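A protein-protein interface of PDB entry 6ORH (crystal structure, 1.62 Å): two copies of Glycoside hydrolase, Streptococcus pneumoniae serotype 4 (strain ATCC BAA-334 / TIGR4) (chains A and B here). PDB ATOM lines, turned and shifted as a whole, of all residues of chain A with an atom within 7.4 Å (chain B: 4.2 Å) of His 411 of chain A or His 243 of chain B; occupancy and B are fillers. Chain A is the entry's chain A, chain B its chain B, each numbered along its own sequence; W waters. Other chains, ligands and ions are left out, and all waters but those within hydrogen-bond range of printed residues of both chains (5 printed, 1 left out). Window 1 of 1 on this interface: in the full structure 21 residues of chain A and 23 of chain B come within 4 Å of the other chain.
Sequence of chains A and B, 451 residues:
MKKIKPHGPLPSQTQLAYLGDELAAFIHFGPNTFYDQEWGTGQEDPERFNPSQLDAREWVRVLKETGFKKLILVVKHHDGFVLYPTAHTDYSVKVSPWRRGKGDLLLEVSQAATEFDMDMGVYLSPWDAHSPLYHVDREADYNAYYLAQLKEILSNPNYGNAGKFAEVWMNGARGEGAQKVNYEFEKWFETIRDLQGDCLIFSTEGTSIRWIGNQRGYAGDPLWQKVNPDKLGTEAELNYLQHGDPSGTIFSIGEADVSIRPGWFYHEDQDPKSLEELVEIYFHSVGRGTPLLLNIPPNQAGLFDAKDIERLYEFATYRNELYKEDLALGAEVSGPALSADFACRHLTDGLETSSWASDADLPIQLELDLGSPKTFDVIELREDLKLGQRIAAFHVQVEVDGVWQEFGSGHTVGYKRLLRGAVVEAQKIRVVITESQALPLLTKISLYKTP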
ATOM      1  N   GLY A 220      -4.711 -18.362 -16.134  1.00  0.00           N
ATOM      2  CA  GLY A 220      -5.342 -17.255 -16.849  1.00  0.00           C
ATOM      3  C   GLY A 220      -5.191 -17.349 -18.372  1.00  0.00           C
ATOM      4  O   GLY A 220      -4.430 -18.155 -18.921  1.00  0.00           O
ATOM      5  N   ASP A 221      -5.978 -16.491 -19.042  1.00  0.00           N
ATOM      6  CA  ASP A 221      -5.755 -16.187 -20.446  1.00  0.00           C
ATOM      7  C   ASP A 221      -5.672 -14.669 -20.506  1.00  0.00           C
ATOM      8  O   ASP A 221      -6.672 -14.002 -20.237  1.00  0.00           O
ATOM      9  CB  ASP A 221      -6.839 -16.788 -21.340  1.00  0.00           C
ATOM     10  CG  ASP A 221      -6.487 -16.767 -22.826  1.00  0.00           C
ATOM     11  OD1 ASP A 221      -5.294 -16.849 -23.142  1.00  0.00           O
ATOM     12  OD2 ASP A 221      -7.418 -16.708 -23.642  1.00  0.00           O
ATOM     13  N   PRO A 222      -4.504 -14.073 -20.794  1.00  0.00           N
ATOM     14  CA  PRO A 222      -3.309 -14.776 -21.260  1.00  0.00           C
ATOM     15  C   PRO A 222      -2.606 -15.554 -20.148  1.00  0.00           C
ATOM     16  O   PRO A 222      -2.779 -15.240 -18.972  1.00  0.00           O
ATOM     17  CB  PRO A 222      -2.355 -13.633 -21.670  1.00  0.00           C
ATOM     18  CG  PRO A 222      -2.817 -12.437 -20.837  1.00  0.00           C
ATOM     19  CD  PRO A 222      -4.304 -12.610 -20.758  1.00  0.00           C
ATOM     20  N   LEU A 223      -1.839 -16.583 -20.551  1.00  0.00           N
ATOM     21  CA  LEU A 223      -0.835 -17.163 -19.661  1.00  0.00           C
ATOM     22  C   LEU A 223       0.528 -17.054 -20.327  1.00  0.00           C
ATOM     23  O   LEU A 223       0.864 -17.857 -21.212  1.00  0.00           O
ATOM     24  CB  LEU A 223      -1.145 -18.622 -19.272  1.00  0.00           C
ATOM     25  CG  LEU A 223      -0.027 -19.275 -18.423  1.00  0.00           C
ATOM     26  CD1 LEU A 223       0.150 -18.566 -17.075  1.00  0.00           C
ATOM     27  CD2 LEU A 223      -0.230 -20.789 -18.232  1.00  0.00           C
ATOM     28  N   TRP A 224       1.308 -16.054 -19.889  1.00  0.00           N
ATOM     29  CA  TRP A 224       2.723 -15.968 -20.228  1.00  0.00           C
ATOM     30  C   TRP A 224       3.513 -16.804 -19.225  1.00  0.00           C
ATOM     31  O   TRP A 224       3.387 -16.600 -18.001  1.00  0.00           O
ATOM     32  CB  TRP A 224       3.170 -14.493 -20.189  1.00  0.00           C
ATOM     33  CG  TRP A 224       2.428 -13.653 -21.182  1.00  0.00           C
ATOM     34  CD1 TRP A 224       1.357 -12.814 -20.994  1.00  0.00           C
ATOM     35  CD2 TRP A 224       2.752 -13.589 -22.583  1.00  0.00           C
ATOM     36  NE1 TRP A 224       0.980 -12.232 -22.190  1.00  0.00           N
ATOM     37  CE2 TRP A 224       1.835 -12.692 -23.169  1.00  0.00           C
ATOM     38  CE3 TRP A 224       3.720 -14.243 -23.375  1.00  0.00           C
ATOM     39  CZ2 TRP A 224       1.836 -12.434 -24.543  1.00  0.00           C
ATOM     40  CZ3 TRP A 224       3.759 -13.946 -24.729  1.00  0.00           C
ATOM     41  CH2 TRP A 224       2.834 -13.047 -25.282  1.00  0.00           C
ATOM     42  N   HIS A 243      -1.392 -14.904 -14.780  1.00  0.00           N
ATOM     43  CA  HIS A 243      -1.275 -14.554 -16.195  1.00  0.00           C
ATOM     44  C   HIS A 243       0.180 -14.462 -16.637  1.00  0.00           C
ATOM     45  O   HIS A 243       0.444 -14.347 -17.839  1.00  0.00           O
ATOM     46  CB  HIS A 243      -1.946 -13.203 -16.494  1.00  0.00           C
ATOM     47  CG  HIS A 243      -3.409 -13.223 -16.254  1.00  0.00           C
ATOM     48  ND1 HIS A 243      -4.304 -13.751 -17.182  1.00  0.00           N
ATOM     49  CD2 HIS A 243      -4.167 -12.772 -15.213  1.00  0.00           C
ATOM     50  CE1 HIS A 243      -5.545 -13.661 -16.734  1.00  0.00           C
ATOM     51  NE2 HIS A 243      -5.486 -13.081 -15.506  1.00  0.00           N
ATOM     52  N   GLU A 383       2.962 -23.668 -29.824  1.00  0.00           N
ATOM     53  CA  GLU A 383       4.111 -22.871 -30.222  1.00  0.00           C
ATOM     54  C   GLU A 383       5.382 -23.702 -30.156  1.00  0.00           C
ATOM     55  O   GLU A 383       5.356 -24.848 -29.723  1.00  0.00           O
ATOM     56  CB  GLU A 383       4.290 -21.621 -29.348  1.00  0.00           C
ATOM     57  CG  GLU A 383       3.342 -20.528 -29.745  1.00  0.00           C
ATOM     58  CD  GLU A 383       3.532 -19.256 -28.943  1.00  0.00           C
ATOM     59  OE1 GLU A 383       3.048 -19.227 -27.780  1.00  0.00           O
ATOM     60  OE2 GLU A 383       4.052 -18.279 -29.519  1.00  0.00           O
ATOM     61  N   GLN A 389       8.158 -17.887 -26.221  1.00  0.00           N
ATOM     62  CA  GLN A 389       6.718 -17.693 -26.364  1.00  0.00           C
ATOM     63  C   GLN A 389       6.441 -16.336 -27.016  1.00  0.00           C
ATOM     64  O   GLN A 389       7.047 -15.315 -26.634  1.00  0.00           O
ATOM     65  CB  GLN A 389       6.099 -17.715 -24.955  1.00  0.00           C
ATOM     66  CG  GLN A 389       4.569 -17.719 -24.955  1.00  0.00           C
ATOM     67  CD  GLN A 389       3.949 -17.855 -23.580  1.00  0.00           C
ATOM     68  OE1 GLN A 389       4.669 -17.957 -22.582  1.00  0.00           O
ATOM     69  NE2 GLN A 389       2.617 -17.879 -23.532  1.00  0.00           N
ATOM     70  N   ARG A 390       5.497 -16.290 -27.972  1.00  0.00           N
ATOM     71  CA  ARG A 390       5.352 -15.092 -28.800  1.00  0.00           C
ATOM     72  C   ARG A 390       3.912 -14.624 -28.963  1.00  0.00           C
ATOM     73  O   ARG A 390       3.648 -13.421 -28.885  1.00  0.00           O
ATOM     74  CB  ARG A 390       5.938 -15.359 -30.205  1.00  0.00           C
ATOM     75  CG  ARG A 390       7.410 -15.762 -30.187  1.00  0.00           C
ATOM     76  CD  ARG A 390       7.881 -16.357 -31.534  1.00  0.00           C
ATOM     77  NE  ARG A 390       9.283 -16.662 -31.390  1.00  0.00           N
ATOM     78  CZ  ARG A 390      10.267 -16.276 -32.212  1.00  0.00           C
ATOM     79  NH1 ARG A 390       9.995 -15.625 -33.340  1.00  0.00           N
ATOM     80  NH2 ARG A 390      11.509 -16.589 -31.913  1.00  0.00           N
ATOM     81  N   ILE A 391       2.969 -15.554 -29.204  1.00  0.00           N
ATOM     82  CA  ILE A 391       1.630 -15.162 -29.635  1.00  0.00           C
ATOM     83  C   ILE A 391       0.872 -14.522 -28.480  1.00  0.00           C
ATOM     84  O   ILE A 391       0.879 -15.077 -27.386  1.00  0.00           O
ATOM     85  CB  ILE A 391       0.863 -16.363 -30.218  1.00  0.00           C
ATOM     86  CG1 ILE A 391       1.515 -16.751 -31.546  1.00  0.00           C
ATOM     87  CG2 ILE A 391      -0.611 -16.016 -30.411  1.00  0.00           C
ATOM     88  CD1 ILE A 391       1.086 -18.137 -32.055  1.00  0.00           C
ATOM     89  N   ALA A 392       0.217 -13.395 -28.754  1.00  0.00           N
ATOM     90  CA  ALA A 392      -0.526 -12.671 -27.735  1.00  0.00           C
ATOM     91  C   ALA A 392      -2.018 -12.583 -28.041  1.00  0.00           C
ATOM     92  O   ALA A 392      -2.805 -12.199 -27.159  1.00  0.00           O
ATOM     93  CB  ALA A 392       0.086 -11.284 -27.575  1.00  0.00           C
ATOM     94  N   ALA A 393      -2.433 -12.883 -29.295  1.00  0.00           N
ATOM     95  CA  ALA A 393      -3.861 -12.897 -29.598  1.00  0.00           C
ATOM     96  C   ALA A 393      -4.108 -13.696 -30.867  1.00  0.00           C
ATOM     97  O   ALA A 393      -3.350 -13.569 -31.829  1.00  0.00           O
ATOM     98  CB  ALA A 393      -4.408 -11.495 -29.799  1.00  0.00           C
ATOM     99  N   PHE A 394      -5.176 -14.491 -30.844  1.00  0.00           N
ATOM    100  CA  PHE A 394      -5.539 -15.242 -32.048  1.00  0.00           C
ATOM    101  C   PHE A 394      -7.043 -15.507 -32.021  1.00  0.00           C
ATOM    102  O   PHE A 394      -7.691 -15.438 -30.968  1.00  0.00           O
ATOM    103  CB  PHE A 394      -4.714 -16.540 -32.144  1.00  0.00           C
ATOM    104  CG  PHE A 394      -5.146 -17.565 -31.123  1.00  0.00           C
ATOM    105  CD1 PHE A 394      -4.673 -17.476 -29.814  1.00  0.00           C
ATOM    106  CD2 PHE A 394      -6.125 -18.512 -31.413  1.00  0.00           C
ATOM    107  CE1 PHE A 394      -5.161 -18.327 -28.830  1.00  0.00           C
ATOM    108  CE2 PHE A 394      -6.616 -19.360 -30.431  1.00  0.00           C
ATOM    109  CZ  PHE A 394      -6.098 -19.297 -29.140  1.00  0.00           C
ATOM    110  N   HIS A 395      -7.626 -15.855 -33.181  1.00  0.00           N
ATOM    111  CA  HIS A 395      -8.991 -16.344 -33.177  1.00  0.00           C
ATOM    112  C   HIS A 395      -9.122 -17.448 -34.226  1.00  0.00           C
ATOM    113  O   HIS A 395      -8.240 -17.632 -35.061  1.00  0.00           O
ATOM    114  CB  HIS A 395     -10.028 -15.210 -33.330  1.00  0.00           C
ATOM    115  CG  HIS A 395      -9.945 -14.442 -34.608  1.00  0.00           C
ATOM    116  ND1 HIS A 395      -9.080 -13.372 -34.761  1.00  0.00           N
ATOM    117  CD2 HIS A 395     -10.625 -14.562 -35.780  1.00  0.00           C
ATOM    118  CE1 HIS A 395      -9.212 -12.877 -35.984  1.00  0.00           C
ATOM    119  NE2 HIS A 395     -10.153 -13.591 -36.620  1.00  0.00           N
ATOM    120  N   SER A 409     -11.839 -17.565 -29.503  1.00  0.00           N
ATOM    121  CA  SER A 409     -10.680 -16.688 -29.541  1.00  0.00           C
ATOM    122  C   SER A 409      -9.898 -16.864 -28.249  1.00  0.00           C
ATOM    123  O   SER A 409     -10.406 -17.405 -27.258  1.00  0.00           O
ATOM    124  CB  SER A 409     -11.065 -15.225 -29.713  1.00  0.00           C
ATOM    125  OG  SER A 409     -11.755 -14.742 -28.568  1.00  0.00           O
ATOM    126  N   GLY A 410      -8.684 -16.322 -28.272  1.00  0.00           N
ATOM    127  CA  GLY A 410      -7.835 -16.391 -27.094  1.00  0.00           C
ATOM    128  C   GLY A 410      -6.726 -15.355 -27.133  1.00  0.00           C
ATOM    129  O   GLY A 410      -6.595 -14.554 -28.075  1.00  0.00           O
ATOM    130  N   HIS A 411      -5.933 -15.361 -26.063  1.00  0.00           N
ATOM    131  CA  HIS A 411      -4.733 -14.551 -26.016  1.00  0.00           C
ATOM    132  C   HIS A 411      -3.521 -15.391 -26.418  1.00  0.00           C
ATOM    133  O   HIS A 411      -3.089 -15.355 -27.580  1.00  0.00           O
ATOM    134  CB  HIS A 411      -4.555 -13.965 -24.597  1.00  0.00           C
ATOM    135  CG  HIS A 411      -5.595 -12.981 -24.200  1.00  0.00           C
ATOM    136  ND1 HIS A 411      -5.332 -11.626 -24.107  1.00  0.00           N
ATOM    137  CD2 HIS A 411      -6.878 -13.145 -23.832  1.00  0.00           C
ATOM    138  CE1 HIS A 411      -6.428 -11.002 -23.705  1.00  0.00           C
ATOM    139  NE2 HIS A 411      -7.387 -11.906 -23.537  1.00  0.00           N
ATOM    140  N   THR A 412      -2.954 -16.131 -25.449  1.00  0.00           N
ATOM    141  CA  THR A 412      -1.727 -16.891 -25.652  1.00  0.00           C
ATOM    142  C   THR A 412      -2.006 -18.287 -26.220  1.00  0.00           C
ATOM    143  O   THR A 412      -3.131 -18.811 -26.183  1.00  0.00           O
ATOM    144  CB  THR A 412      -0.954 -17.014 -24.325  1.00  0.00           C
ATOM    145  OG1 THR A 412      -1.910 -17.403 -23.319  1.00  0.00           O
ATOM    146  CG2 THR A 412      -0.319 -15.698 -23.915  1.00  0.00           C
ATOM    147  N   VAL A 413      -0.932 -18.876 -26.741  1.00  0.00           N
ATOM    148  CA  VAL A 413      -0.921 -20.273 -27.136  1.00  0.00           C
ATOM    149  C   VAL A 413      -0.017 -21.014 -26.149  1.00  0.00           C
ATOM    150  O   VAL A 413      -0.497 -21.856 -25.385  1.00  0.00           O
ATOM    151  CB  VAL A 413      -0.473 -20.395 -28.611  1.00  0.00           C
ATOM    152  CG1 VAL A 413      -0.240 -21.864 -28.988  1.00  0.00           C
ATOM    153  CG2 VAL A 413      -1.533 -19.811 -29.562  1.00  0.00           C
ATOM    154  N   GLY A 414       1.288 -20.722 -26.166  1.00  0.00           N
ATOM    155  CA  GLY A 414       2.216 -21.378 -25.255  1.00  0.00           C
ATOM    156  C   GLY A 414       2.603 -22.782 -25.742  1.00  0.00           C
ATOM    157  O   GLY A 414       2.547 -23.074 -26.947  1.00  0.00           O
ATOM    158  N   ARG A 417      -2.283 -25.144 -26.402  1.00  0.00           N
ATOM    159  CA  ARG A 417      -3.527 -24.464 -26.088  1.00  0.00           C
ATOM    160  C   ARG A 417      -4.658 -25.300 -26.680  1.00  0.00           C
ATOM    161  O   ARG A 417      -4.631 -25.614 -27.877  1.00  0.00           O
ATOM    162  CB  ARG A 417      -3.537 -23.070 -26.751  1.00  0.00           C
ATOM    163  CG  ARG A 417      -4.805 -22.249 -26.549  1.00  0.00           C
ATOM    164  CD  ARG A 417      -4.951 -21.829 -25.086  1.00  0.00           C
ATOM    165  NE  ARG A 417      -6.269 -21.292 -24.746  1.00  0.00           N
ATOM    166  CZ  ARG A 417      -6.559 -20.008 -24.619  1.00  0.00           C
ATOM    167  NH1 ARG A 417      -5.679 -19.051 -24.935  1.00  0.00           N
ATOM    168  NH2 ARG A 417      -7.780 -19.680 -24.217  1.00  0.00           N
ATOM    169  N   LEU A 419      -8.613 -25.022 -27.324  1.00  0.00           N
ATOM    170  CA  LEU A 419      -9.714 -24.085 -27.279  1.00  0.00           C
ATOM    171  C   LEU A 419     -11.016 -24.765 -27.721  1.00  0.00           C
ATOM    172  O   LEU A 419     -11.077 -25.283 -28.830  1.00  0.00           O
ATOM    173  CB  LEU A 419      -9.348 -22.929 -28.213  1.00  0.00           C
ATOM    174  CG  LEU A 419     -10.396 -21.826 -28.290  1.00  0.00           C
ATOM    175  CD1 LEU A 419     -10.444 -21.040 -26.971  1.00  0.00           C
ATOM    176  CD2 LEU A 419     -10.027 -20.901 -29.446  1.00  0.00           C
ATOM    177  N   THR A 434      -3.323 -12.475 -34.583  1.00  0.00           N
ATOM    178  CA  THR A 434      -3.601 -11.043 -34.695  1.00  0.00           C
ATOM    179  C   THR A 434      -2.606 -10.190 -33.911  1.00  0.00           C
ATOM    180  O   THR A 434      -2.448  -8.987 -34.165  1.00  0.00           O
ATOM    181  CB  THR A 434      -5.060 -10.709 -34.357  1.00  0.00           C
ATOM    182  OG1 THR A 434      -5.305 -10.986 -32.963  1.00  0.00           O
ATOM    183  CG2 THR A 434      -6.034 -11.465 -35.235  1.00  0.00           C
ATOM    184  N   GLU A 435      -1.945 -10.797 -32.924  1.00  0.00           N
ATOM    185  CA  GLU A 435      -0.909 -10.082 -32.185  1.00  0.00           C
ATOM    186  C   GLU A 435       0.181 -11.058 -31.743  1.00  0.00           C
ATOM    187  O   GLU A 435      -0.125 -12.168 -31.315  1.00  0.00           O
ATOM    188  CB  GLU A 435      -1.518  -9.378 -30.960  1.00  0.00           C
ATOM    189  CG  GLU A 435      -0.519  -8.422 -30.349  1.00  0.00           C
ATOM    190  CD  GLU A 435      -1.012  -7.729 -29.098  1.00  0.00           C
ATOM    191  OE1 GLU A 435      -2.107  -7.137 -29.169  1.00  0.00           O
ATOM    192  OE2 GLU A 435      -0.248  -7.706 -28.085  1.00  0.00           O
ATOM    193  N   GLY B 220     -14.903 -10.351 -21.136  1.00  0.00           N
ATOM    194  CA  GLY B 220     -13.623 -10.677 -20.525  1.00  0.00           C
ATOM    195  C   GLY B 220     -13.523 -10.314 -19.045  1.00  0.00           C
ATOM    196  O   GLY B 220     -14.364  -9.602 -18.494  1.00  0.00           O
ATOM    197  N   ASP B 221     -12.478 -10.858 -18.406  1.00  0.00           N
ATOM    198  CA  ASP B 221     -12.035 -10.357 -17.118  1.00  0.00           C
ATOM    199  C   ASP B 221     -10.554 -10.059 -17.278  1.00  0.00           C
ATOM    200  O   ASP B 221      -9.765 -10.967 -17.518  1.00  0.00           O
ATOM    201  CB  ASP B 221     -12.321 -11.345 -15.983  1.00  0.00           C
ATOM    202  CG  ASP B 221     -12.094 -10.736 -14.598  1.00  0.00           C
ATOM    203  OD1 ASP B 221     -12.323  -9.521 -14.454  1.00  0.00           O
ATOM    204  OD2 ASP B 221     -11.745 -11.488 -13.661  1.00  0.00           O
ATOM    205  N   PRO B 222     -10.114  -8.788 -17.259  1.00  0.00           N
ATOM    206  CA  PRO B 222     -10.961  -7.646 -16.916  1.00  0.00           C
ATOM    207  C   PRO B 222     -12.005  -7.292 -17.963  1.00  0.00           C
ATOM    208  O   PRO B 222     -11.804  -7.584 -19.158  1.00  0.00           O
ATOM    209  CB  PRO B 222      -9.910  -6.497 -16.874  1.00  0.00           C
ATOM    210  CG  PRO B 222      -8.833  -6.920 -17.858  1.00  0.00           C
ATOM    211  CD  PRO B 222      -8.762  -8.421 -17.712  1.00  0.00           C
ATOM    212  N   LEU B 223     -13.079  -6.587 -17.521  1.00  0.00           N
ATOM    213  CA  LEU B 223     -13.922  -5.832 -18.445  1.00  0.00           C
ATOM    214  C   LEU B 223     -13.952  -4.356 -18.048  1.00  0.00           C
ATOM    215  O   LEU B 223     -14.583  -3.978 -17.049  1.00  0.00           O
ATOM    216  CB  LEU B 223     -15.345  -6.397 -18.530  1.00  0.00           C
ATOM    217  CG  LEU B 223     -16.263  -5.525 -19.383  1.00  0.00           C
ATOM    218  CD1 LEU B 223     -15.801  -5.479 -20.831  1.00  0.00           C
ATOM    219  CD2 LEU B 223     -17.706  -6.021 -19.321  1.00  0.00           C
ATOM    220  N   TRP B 224     -13.162  -3.566 -18.797  1.00  0.00           N
ATOM    221  CA  TRP B 224     -13.202  -2.127 -18.658  1.00  0.00           C
ATOM    222  C   TRP B 224     -14.289  -1.634 -19.608  1.00  0.00           C
ATOM    223  O   TRP B 224     -14.274  -1.917 -20.811  1.00  0.00           O
ATOM    224  CB  TRP B 224     -11.828  -1.506 -18.986  1.00  0.00           C
ATOM    225  CG  TRP B 224     -10.754  -1.918 -18.023  1.00  0.00           C
ATOM    226  CD1 TRP B 224      -9.777  -2.863 -18.223  1.00  0.00           C
ATOM    227  CD2 TRP B 224     -10.566  -1.415 -16.684  1.00  0.00           C
ATOM    228  NE1 TRP B 224      -9.002  -2.988 -17.095  1.00  0.00           N
ATOM    229  CE2 TRP B 224      -9.454  -2.099 -16.146  1.00  0.00           C
ATOM    230  CE3 TRP B 224     -11.234  -0.466 -15.877  1.00  0.00           C
ATOM    231  CZ2 TRP B 224      -8.985  -1.873 -14.849  1.00  0.00           C
ATOM    232  CZ3 TRP B 224     -10.758  -0.228 -14.593  1.00  0.00           C
ATOM    233  CH2 TRP B 224      -9.653  -0.926 -14.096  1.00  0.00           C
ATOM    234  N   ASN B 239      -9.786  -8.875 -28.646  1.00  0.00           N
ATOM    235  CA  ASN B 239      -9.499  -8.828 -27.210  1.00  0.00           C
ATOM    236  C   ASN B 239      -9.686  -7.424 -26.635  1.00  0.00           C
ATOM    237  O   ASN B 239      -9.999  -7.279 -25.452  1.00  0.00           O
ATOM    238  CB  ASN B 239      -8.087  -9.344 -26.902  1.00  0.00           C
ATOM    239  CG  ASN B 239      -7.988 -10.844 -27.097  1.00  0.00           C
ATOM    240  OD1 ASN B 239      -9.011 -11.508 -27.142  1.00  0.00           O
ATOM    241  ND2 ASN B 239      -6.783 -11.382 -27.146  1.00  0.00           N
ATOM    242  N   TYR B 240      -9.438  -6.413 -27.460  1.00  0.00           N
ATOM    243  CA  TYR B 240      -9.667  -5.028 -27.077  1.00  0.00           C
ATOM    244  C   TYR B 240     -11.148  -4.781 -26.800  1.00  0.00           C
ATOM    245  O   TYR B 240     -11.513  -4.143 -25.817  1.00  0.00           O
ATOM    246  CB  TYR B 240      -9.132  -4.091 -28.150  1.00  0.00           C
ATOM    247  CG  TYR B 240      -9.162  -2.648 -27.735  1.00  0.00           C
ATOM    248  CD1 TYR B 240      -8.218  -2.170 -26.832  1.00  0.00           C
ATOM    249  CD2 TYR B 240     -10.113  -1.774 -28.252  1.00  0.00           C
ATOM    250  CE1 TYR B 240      -8.220  -0.828 -26.467  1.00  0.00           C
ATOM    251  CE2 TYR B 240     -10.128  -0.436 -27.880  1.00  0.00           C
ATOM    252  CZ  TYR B 240      -9.194   0.017 -26.961  1.00  0.00           C
ATOM    253  OH  TYR B 240      -9.184   1.344 -26.606  1.00  0.00           O
ATOM    254  N   LEU B 241     -12.012  -5.252 -27.704  1.00  0.00           N
ATOM    255  CA  LEU B 241     -13.447  -5.164 -27.469  1.00  0.00           C
ATOM    256  C   LEU B 241     -13.880  -5.947 -26.229  1.00  0.00           C
ATOM    257  O   LEU B 241     -14.725  -5.488 -25.459  1.00  0.00           O
ATOM    258  CB  LEU B 241     -14.191  -5.679 -28.708  1.00  0.00           C
ATOM    259  CG  LEU B 241     -13.911  -4.940 -30.013  1.00  0.00           C
ATOM    260  CD1 LEU B 241     -14.623  -5.655 -31.187  1.00  0.00           C
ATOM    261  CD2 LEU B 241     -14.359  -3.481 -29.889  1.00  0.00           C
ATOM    262  N   GLN B 242     -13.292  -7.138 -26.028  1.00  0.00           N
ATOM    263  CA  GLN B 242     -13.721  -8.078 -25.013  1.00  0.00           C
ATOM    264  C   GLN B 242     -13.315  -7.635 -23.608  1.00  0.00           C
ATOM    265  O   GLN B 242     -14.014  -7.932 -22.640  1.00  0.00           O
ATOM    266  CB  GLN B 242     -13.053  -9.418 -25.317  1.00  0.00           C
ATOM    267  CG  GLN B 242     -13.362 -10.535 -24.323  1.00  0.00           C
ATOM    268  CD  GLN B 242     -12.828 -11.824 -24.895  1.00  0.00           C
ATOM    269  OE1 GLN B 242     -13.427 -12.425 -25.801  1.00  0.00           O
ATOM    270  NE2 GLN B 242     -11.661 -12.247 -24.418  1.00  0.00           N
ATOM    271  N   HIS B 243     -12.215  -6.877 -23.504  1.00  0.00           N
ATOM    272  CA  HIS B 243     -11.702  -6.476 -22.200  1.00  0.00           C
ATOM    273  C   HIS B 243     -11.779  -4.965 -21.994  1.00  0.00           C
ATOM    274  O   HIS B 243     -11.571  -4.509 -20.868  1.00  0.00           O
ATOM    275  CB  HIS B 243     -10.240  -6.912 -22.023  1.00  0.00           C
ATOM    276  CG  HIS B 243     -10.089  -8.393 -22.015  1.00  0.00           C
ATOM    277  ND1 HIS B 243     -10.327  -9.164 -20.878  1.00  0.00           N
ATOM    278  CD2 HIS B 243      -9.691  -9.243 -22.992  1.00  0.00           C
ATOM    279  CE1 HIS B 243     -10.103 -10.445 -21.165  1.00  0.00           C
ATOM    280  NE2 HIS B 243      -9.708 -10.501 -22.459  1.00  0.00           N
ATOM    281  N   GLY B 244     -12.043  -4.211 -23.063  1.00  0.00           N
ATOM    282  CA  GLY B 244     -11.966  -2.755 -22.975  1.00  0.00           C
ATOM    283  C   GLY B 244     -10.514  -2.322 -22.759  1.00  0.00           C
ATOM    284  O   GLY B 244      -9.584  -3.123 -22.850  1.00  0.00           O
ATOM    285  N   ASP B 245     -10.376  -1.044 -22.390  1.00  0.00           N
ATOM    286  CA  ASP B 245      -9.103  -0.342 -22.354  1.00  0.00           C
ATOM    287  C   ASP B 245      -8.929   0.248 -20.964  1.00  0.00           C
ATOM    288  O   ASP B 245      -9.727   1.089 -20.588  1.00  0.00           O
ATOM    289  CB  ASP B 245      -9.110   0.788 -23.393  1.00  0.00           C
ATOM    290  CG  ASP B 245      -7.748   1.447 -23.620  1.00  0.00           C
ATOM    291  OD1 ASP B 245      -6.892   1.329 -22.725  1.00  0.00           O
ATOM    292  OD2 ASP B 245      -7.573   2.051 -24.723  1.00  0.00           O
HETATM  293  O   HOH W   1     -13.497 -15.152 -26.136  1.00  0.00           O
HETATM  294  O   HOH W   2      -7.371 -11.528 -19.056  1.00  0.00           O
HETATM  295  O   HOH W   3      -4.684  -9.390 -26.829  1.00  0.00           O
HETATM  296  O   HOH W   4     -13.523 -12.627 -28.563  1.00  0.00           O
HETATM  297  O   HOH W   5      -9.990 -13.938 -26.328  1.00  0.00           O
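A ring nitrogen (ND1) of His 411 of chain A sits at hydrogen-bond distance from the side-chain amide nitrogen (ND2) of Asn 239 of chain B, 3.4 Å away.
ND2 of Asn 239 of chain B sits at hydrogen-bond distance from O of Gly 410 of chain A (3.3 Å).
A ring nitrogen (NE2) of His 411 of chain A sits at hydrogen-bond distance from a ring nitrogen (NE2) of His 243 of chain B (2.9 Å).
N of Trp 224 of chain B lies within hydrogen-bond range of O of His 243 of chain B (2.8 Å).
The backbone NH of Ala 393 of chain A lies within hydrogen-bond range of the backbone carbonyl oxygen of Glu 435 of chain A, at 3.1 Å.
ND1 of His 243 of chain B is in hydrogen-bond range of O of Pro 222 of chain B.
N of Gly 220 of chain B is in hydrogen-bond range of O of Gln 242 of chain B, 3.0 Å away.
The side-chain amide nitrogen of Gln 242 of chain B sits at hydrogen-bond distance from a ring nitrogen (NE2) of His 243 of chain B (3.3 Å).
Among the printed residues, merely in contact across the chains: Ala 393 of chain A with Asn 239 of chain B (3.6 Å) and Ser 409 of chain A with Gln 242 of chain B (3.98 Å).
Of the printed residues of chain B, Ala 393 of chain A touches Asn 239.
Of the printed residues of chain B, Ser 409 of chain A touches Gln 242 (3.98 Å).
Of the printed residues of chain B, Gly 410 of chain A touches Asn 239 (3.3 Å).
His 411 of chain A touches two residues of chain B.
Printed residues of chain A within 4 Å of Gln 242 of chain B: Ser 409 (3.98 Å).
His 243 of chain B touches just one residue of chain A: His 411.
No residue of chain A comes within 4 Å of Gly 244 of chain B.
Asp 245 of chain B touches none of the printed residues of chain A.
The nearest printed residue of chain B that does not touch His 411 of chain A is Gln 242 of chain B (4.4 Å).
The nearest residue of chain A that does not touch His 243 of chain B is Asp 221 of chain A (5.0 Å).
The nearest printed residue of chain B that does not touch Ser 409 of chain A is Asn 239 of chain B (4.5 Å).
Of the 24 printed residues of chain A, 4 touch a printed residue of chain B.
Hydrophobic or aromatic side chains of chain B within 4 Å of the printed part of chain A: His 243.
Among the printed residues, 5 pairs touch across the chains.
Positions printed for both chains: 220, 221, 222, 223, 224 and 243.
Of the 5 pairs that touch across the chains among the printed residues, none has its exchanged pair printed and touching as well.
Water W5 lies within hydrogen-bond range of the side-chain amide oxygen (OD1) of Asn 239 of chain B (2.7 Å), the side-chain hydroxyl (OG) of Ser 409 of chain A (3.0 Å), the side-chain amide nitrogen (NE2) of Gln 242 of chain B (3.0 Å) and the backbone NH (N) of Gly 410 of chain A (3.3 Å).
Water W4 lies within hydrogen-bond range of the side-chain hydroxyl (OG) of Ser 409 of chain A and the side-chain amide oxygen (OE1) of Gln 242 of chain B.
Water W3 lies within hydrogen-bond range of ND2 of Asn 239 of chain B and O of Ala 392 of chain A.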
